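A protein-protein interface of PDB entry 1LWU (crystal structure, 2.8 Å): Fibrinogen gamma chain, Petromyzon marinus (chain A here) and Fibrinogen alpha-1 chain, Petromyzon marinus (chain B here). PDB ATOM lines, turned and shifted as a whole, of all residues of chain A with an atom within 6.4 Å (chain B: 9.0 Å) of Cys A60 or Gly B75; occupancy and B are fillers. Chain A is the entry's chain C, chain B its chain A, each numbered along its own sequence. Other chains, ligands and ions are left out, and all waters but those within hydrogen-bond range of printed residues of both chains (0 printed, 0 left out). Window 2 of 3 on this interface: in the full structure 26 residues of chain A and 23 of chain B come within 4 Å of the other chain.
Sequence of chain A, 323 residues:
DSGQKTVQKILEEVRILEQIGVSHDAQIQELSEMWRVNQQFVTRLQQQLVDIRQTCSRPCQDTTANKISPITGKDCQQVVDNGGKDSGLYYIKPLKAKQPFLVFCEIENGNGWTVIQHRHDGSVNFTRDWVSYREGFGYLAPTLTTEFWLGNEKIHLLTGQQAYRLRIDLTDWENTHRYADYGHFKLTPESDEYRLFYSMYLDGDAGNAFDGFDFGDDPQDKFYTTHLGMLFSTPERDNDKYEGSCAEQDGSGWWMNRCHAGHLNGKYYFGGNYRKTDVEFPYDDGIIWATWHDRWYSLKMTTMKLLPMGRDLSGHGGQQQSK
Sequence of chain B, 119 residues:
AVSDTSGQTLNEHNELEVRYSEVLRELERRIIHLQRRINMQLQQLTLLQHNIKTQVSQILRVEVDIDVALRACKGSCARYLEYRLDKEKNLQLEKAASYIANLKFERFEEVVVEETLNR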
ATOM      1  N   CYS A  56      -7.229  -4.577   4.177  1.00  0.00           N
ATOM      2  CA  CYS A  56      -8.038  -3.841   5.135  1.00  0.00           C
ATOM      3  C   CYS A  56      -9.094  -4.648   5.875  1.00  0.00           C
ATOM      4  O   CYS A  56     -10.059  -4.078   6.394  1.00  0.00           O
ATOM      5  CB  CYS A  56      -8.674  -2.625   4.458  1.00  0.00           C
ATOM      6  SG  CYS A  56      -7.424  -1.427   3.922  1.00  0.00           S
ATOM      7  N   ARG A  58      -8.297  -6.804   8.534  1.00  0.00           N
ATOM      8  CA  ARG A  58      -7.891  -6.978   9.922  1.00  0.00           C
ATOM      9  C   ARG A  58      -8.231  -5.729  10.733  1.00  0.00           C
ATOM     10  O   ARG A  58      -8.118  -4.615  10.238  1.00  0.00           O
ATOM     11  CB  ARG A  58      -6.393  -7.250   9.992  1.00  0.00           C
ATOM     12  CG  ARG A  58      -5.876  -8.148   8.884  1.00  0.00           C
ATOM     13  CD  ARG A  58      -4.416  -8.561   9.103  1.00  0.00           C
ATOM     14  NE  ARG A  58      -4.273  -9.766   9.928  1.00  0.00           N
ATOM     15  CZ  ARG A  58      -4.553  -9.847  11.230  1.00  0.00           C
ATOM     16  NH1 ARG A  58      -4.999  -8.787  11.893  1.00  0.00           N
ATOM     17  NH2 ARG A  58      -4.389 -10.998  11.875  1.00  0.00           N
ATOM     18  N   PRO A  59      -8.670  -5.939  11.900  1.00  0.00           N
ATOM     19  CA  PRO A  59      -8.967  -4.931  12.958  1.00  0.00           C
ATOM     20  C   PRO A  59      -7.810  -4.345  13.724  1.00  0.00           C
ATOM     21  O   PRO A  59      -6.855  -5.058  13.888  1.00  0.00           O
ATOM     22  CB  PRO A  59      -9.970  -5.655  13.847  1.00  0.00           C
ATOM     23  CG  PRO A  59     -10.750  -6.444  12.844  1.00  0.00           C
ATOM     24  CD  PRO A  59      -9.932  -6.620  11.634  1.00  0.00           C
ATOM     25  N   CYS A  60      -7.915  -3.128  14.187  1.00  0.00           N
ATOM     26  CA  CYS A  60      -6.840  -2.599  14.992  1.00  0.00           C
ATOM     27  C   CYS A  60      -6.428  -3.549  16.092  1.00  0.00           C
ATOM     28  O   CYS A  60      -7.227  -4.375  16.548  1.00  0.00           O
ATOM     29  CB  CYS A  60      -7.262  -1.302  15.658  1.00  0.00           C
ATOM     30  SG  CYS A  60      -8.000  -0.120  14.527  1.00  0.00           S
ATOM     31  N   GLN A  61      -5.176  -3.391  16.519  1.00  0.00           N
ATOM     32  CA  GLN A  61      -4.595  -4.163  17.605  1.00  0.00           C
ATOM     33  C   GLN A  61      -4.906  -3.401  18.884  1.00  0.00           C
ATOM     34  O   GLN A  61      -4.649  -2.196  18.979  1.00  0.00           O
ATOM     35  CB  GLN A  61      -3.081  -4.265  17.434  1.00  0.00           C
ATOM     36  CG  GLN A  61      -2.639  -5.227  16.361  1.00  0.00           C
ATOM     37  CD  GLN A  61      -2.984  -6.668  16.707  1.00  0.00           C
ATOM     38  OE1 GLN A  61      -2.485  -7.222  17.692  1.00  0.00           O
ATOM     39  NE2 GLN A  61      -3.844  -7.282  15.898  1.00  0.00           N
ATOM     40  N   ASP A  62      -5.481  -4.094  19.855  1.00  0.00           N
ATOM     41  CA  ASP A  62      -5.803  -3.479  21.131  1.00  0.00           C
ATOM     42  C   ASP A  62      -4.568  -3.678  22.008  1.00  0.00           C
ATOM     43  O   ASP A  62      -4.518  -4.601  22.823  1.00  0.00           O
ATOM     44  CB  ASP A  62      -7.010  -4.178  21.744  1.00  0.00           C
ATOM     45  CG  ASP A  62      -7.505  -3.495  22.983  1.00  0.00           C
ATOM     46  OD1 ASP A  62      -8.544  -3.941  23.508  1.00  0.00           O
ATOM     47  OD2 ASP A  62      -6.864  -2.517  23.431  1.00  0.00           O
ATOM     48  N   ALA B  69     -14.718  -0.655  -0.106  1.00  0.00           N
ATOM     49  CA  ALA B  69     -13.523  -1.292   0.453  1.00  0.00           C
ATOM     50  C   ALA B  69     -12.616  -0.293   1.165  1.00  0.00           C
ATOM     51  O   ALA B  69     -12.330  -0.454   2.352  1.00  0.00           O
ATOM     52  CB  ALA B  69     -12.744  -2.001  -0.640  1.00  0.00           C
ATOM     53  N   LEU B  70     -12.152   0.725   0.440  1.00  0.00           N
ATOM     54  CA  LEU B  70     -11.297   1.750   1.021  1.00  0.00           C
ATOM     55  C   LEU B  70     -11.799   2.235   2.382  1.00  0.00           C
ATOM     56  O   LEU B  70     -11.015   2.480   3.303  1.00  0.00           O
ATOM     57  CB  LEU B  70     -11.218   2.941   0.090  1.00  0.00           C
ATOM     58  CG  LEU B  70      -9.940   3.063  -0.721  1.00  0.00           C
ATOM     59  CD1 LEU B  70      -9.328   1.683  -0.912  1.00  0.00           C
ATOM     60  CD2 LEU B  70     -10.269   3.731  -2.065  1.00  0.00           C
ATOM     61  N   ARG B  71     -13.109   2.386   2.507  1.00  0.00           N
ATOM     62  CA  ARG B  71     -13.679   2.851   3.751  1.00  0.00           C
ATOM     63  C   ARG B  71     -13.370   1.850   4.852  1.00  0.00           C
ATOM     64  O   ARG B  71     -13.241   2.215   6.021  1.00  0.00           O
ATOM     65  CB  ARG B  71     -15.180   3.036   3.559  1.00  0.00           C
ATOM     66  CG  ARG B  71     -15.911   3.639   4.728  1.00  0.00           C
ATOM     67  CD  ARG B  71     -17.210   4.278   4.265  1.00  0.00           C
ATOM     68  NE  ARG B  71     -16.982   5.595   3.670  1.00  0.00           N
ATOM     69  CZ  ARG B  71     -17.109   5.883   2.375  1.00  0.00           C
ATOM     70  NH1 ARG B  71     -17.466   4.951   1.503  1.00  0.00           N
ATOM     71  NH2 ARG B  71     -16.877   7.120   1.953  1.00  0.00           N
ATOM     72  N   ALA B  72     -13.230   0.581   4.465  1.00  0.00           N
ATOM     73  CA  ALA B  72     -12.943  -0.504   5.411  1.00  0.00           C
ATOM     74  C   ALA B  72     -11.626  -0.262   6.142  1.00  0.00           C
ATOM     75  O   ALA B  72     -11.497  -0.592   7.323  1.00  0.00           O
ATOM     76  CB  ALA B  72     -12.912  -1.867   4.673  1.00  0.00           C
ATOM     77  N   CYS B  73     -10.666   0.343   5.441  1.00  0.00           N
ATOM     78  CA  CYS B  73      -9.351   0.614   5.999  1.00  0.00           C
ATOM     79  C   CYS B  73      -9.303   1.515   7.209  1.00  0.00           C
ATOM     80  O   CYS B  73      -8.326   1.495   7.951  1.00  0.00           O
ATOM     81  CB  CYS B  73      -8.455   1.195   4.951  1.00  0.00           C
ATOM     82  SG  CYS B  73      -8.479   0.223   3.442  1.00  0.00           S
ATOM     83  N   LYS B  74     -10.330   2.325   7.408  1.00  0.00           N
ATOM     84  CA  LYS B  74     -10.344   3.197   8.570  1.00  0.00           C
ATOM     85  C   LYS B  74     -10.097   2.333   9.807  1.00  0.00           C
ATOM     86  O   LYS B  74      -9.202   2.600  10.608  1.00  0.00           O
ATOM     87  CB  LYS B  74     -11.697   3.895   8.669  1.00  0.00           C
ATOM     88  CG  LYS B  74     -11.926   4.821   9.870  1.00  0.00           C
ATOM     89  CD  LYS B  74     -13.076   5.793   9.503  1.00  0.00           C
ATOM     90  CE  LYS B  74     -13.541   6.674  10.662  1.00  0.00           C
ATOM     91  NZ  LYS B  74     -14.444   5.975  11.628  1.00  0.00           N
ATOM     92  N   GLY B  75     -10.881   1.274   9.949  1.00  0.00           N
ATOM     93  CA  GLY B  75     -10.716   0.416  11.107  1.00  0.00           C
ATOM     94  C   GLY B  75      -9.631  -0.630  10.955  1.00  0.00           C
ATOM     95  O   GLY B  75      -9.543  -1.532  11.793  1.00  0.00           O
ATOM     96  N   SER B  76      -8.805  -0.517   9.909  1.00  0.00           N
ATOM     97  CA  SER B  76      -7.727  -1.480   9.681  1.00  0.00           C
ATOM     98  C   SER B  76      -6.294  -0.926   9.610  1.00  0.00           C
ATOM     99  O   SER B  76      -5.347  -1.600  10.002  1.00  0.00           O
ATOM    100  CB  SER B  76      -8.016  -2.256   8.410  1.00  0.00           C
ATOM    101  OG  SER B  76      -6.963  -3.147   8.111  1.00  0.00           O
ATOM    102  N   CYS B  77      -6.142   0.300   9.118  1.00  0.00           N
ATOM    103  CA  CYS B  77      -4.829   0.923   8.968  1.00  0.00           C
ATOM    104  C   CYS B  77      -4.504   2.093   9.908  1.00  0.00           C
ATOM    105  O   CYS B  77      -5.391   2.789  10.413  1.00  0.00           O
ATOM    106  CB  CYS B  77      -4.669   1.339   7.509  1.00  0.00           C
ATOM    107  SG  CYS B  77      -5.155  -0.068   6.484  1.00  0.00           S
ATOM    108  N   ALA B  78      -3.208   2.289  10.135  1.00  0.00           N
ATOM    109  CA  ALA B  78      -2.706   3.342  11.009  1.00  0.00           C
ATOM    110  C   ALA B  78      -3.214   4.719  10.585  1.00  0.00           C
ATOM    111  O   ALA B  78      -3.623   5.525  11.424  1.00  0.00           O
ATOM    112  CB  ALA B  78      -1.178   3.316  11.019  1.00  0.00           C
ATOM    113  N   ARG B  79      -3.180   4.990   9.286  1.00  0.00           N
ATOM    114  CA  ARG B  79      -3.658   6.264   8.771  1.00  0.00           C
ATOM    115  C   ARG B  79      -4.757   6.003   7.766  1.00  0.00           C
ATOM    116  O   ARG B  79      -4.664   5.080   6.951  1.00  0.00           O
ATOM    117  CB  ARG B  79      -2.514   7.057   8.119  1.00  0.00           C
ATOM    118  CG  ARG B  79      -1.755   7.937   9.099  1.00  0.00           C
ATOM    119  CD  ARG B  79      -0.280   8.079   8.747  1.00  0.00           C
ATOM    120  NE  ARG B  79      -0.013   8.779   7.488  1.00  0.00           N
ATOM    121  CZ  ARG B  79      -0.500   9.971   7.165  1.00  0.00           C
ATOM    122  NH1 ARG B  79      -1.302  10.610   8.004  1.00  0.00           N
ATOM    123  NH2 ARG B  79      -0.158  10.530   6.017  1.00  0.00           N
ATOM    124  N   TYR B  80      -5.808   6.811   7.840  1.00  0.00           N
ATOM    125  CA  TYR B  80      -6.947   6.674   6.938  1.00  0.00           C
ATOM    126  C   TYR B  80      -7.269   7.985   6.256  1.00  0.00           C
ATOM    127  O   TYR B  80      -7.426   9.009   6.914  1.00  0.00           O
ATOM    128  CB  TYR B  80      -8.195   6.217   7.699  1.00  0.00           C
ATOM    129  CG  TYR B  80      -9.437   6.198   6.831  1.00  0.00           C
ATOM    130  CD1 TYR B  80      -9.521   5.345   5.729  1.00  0.00           C
ATOM    131  CD2 TYR B  80     -10.508   7.050   7.088  1.00  0.00           C
ATOM    132  CE1 TYR B  80     -10.627   5.340   4.904  1.00  0.00           C
ATOM    133  CE2 TYR B  80     -11.623   7.050   6.264  1.00  0.00           C
ATOM    134  CZ  TYR B  80     -11.674   6.190   5.172  1.00  0.00           C
ATOM    135  OH  TYR B  80     -12.769   6.181   4.332  1.00  0.00           O
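Among the printed residues, pairs that only touch across the chains: Cys A56 with Ser B76, Pro A59 with Gly B75, Arg A58 with Gly B75 and Cys A56 with Ala B72.
Of the printed residues of chain B, Cys A60 touches Gly B75 (3.3 Å). Gly B75 touches just these residues of chain A: Arg A58, Pro A59 and Cys A60. Pro A59 touches just one residue of chain B: Gly B75. Of the printed residues of chain A, Ala B72 touches Cys A56. Of the printed residues of chain B, Cys A56 touches Ala B72, Cys B73, Ser B76 and Cys B77. Of the printed residues of chain A, Cys B73 touches Cys A56. Of the printed residues of chain B, Arg A58 touches Gly B75 (3.7 Å) and Ser B76 (2.8 Å).
Of the 12 printed residues of chain B, 5 touch a printed residue of chain A. Hydrophobic or aromatic side chains of chain B within 4 Å of the printed part of chain A: Ala B72. Printed residues of chain A that touch a printed residue of chain B: Cys A56, Arg A58, Pro A59 and Cys A60. Among the printed residues, no Asp or Glu carboxylate lies within 4 Å of a Lys or Arg side-chain nitrogen of the other chain.
SG of Cys B73 is disulfide-bonded to SG of Cys A56 (2.0 Å). The backbone carbonyl oxygen of Gly B75 lies within hydrogen-bond range of the backbone NH of Cys A60, at 3.3 Å. OG of Ser B76 sits at hydrogen-bond distance from O of Arg A58 (2.8 Å). The side-chain sulfur (SG) of Cys B77 sits close to the side-chain sulfur (SG) of Cys A56, at 3.7 Å.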
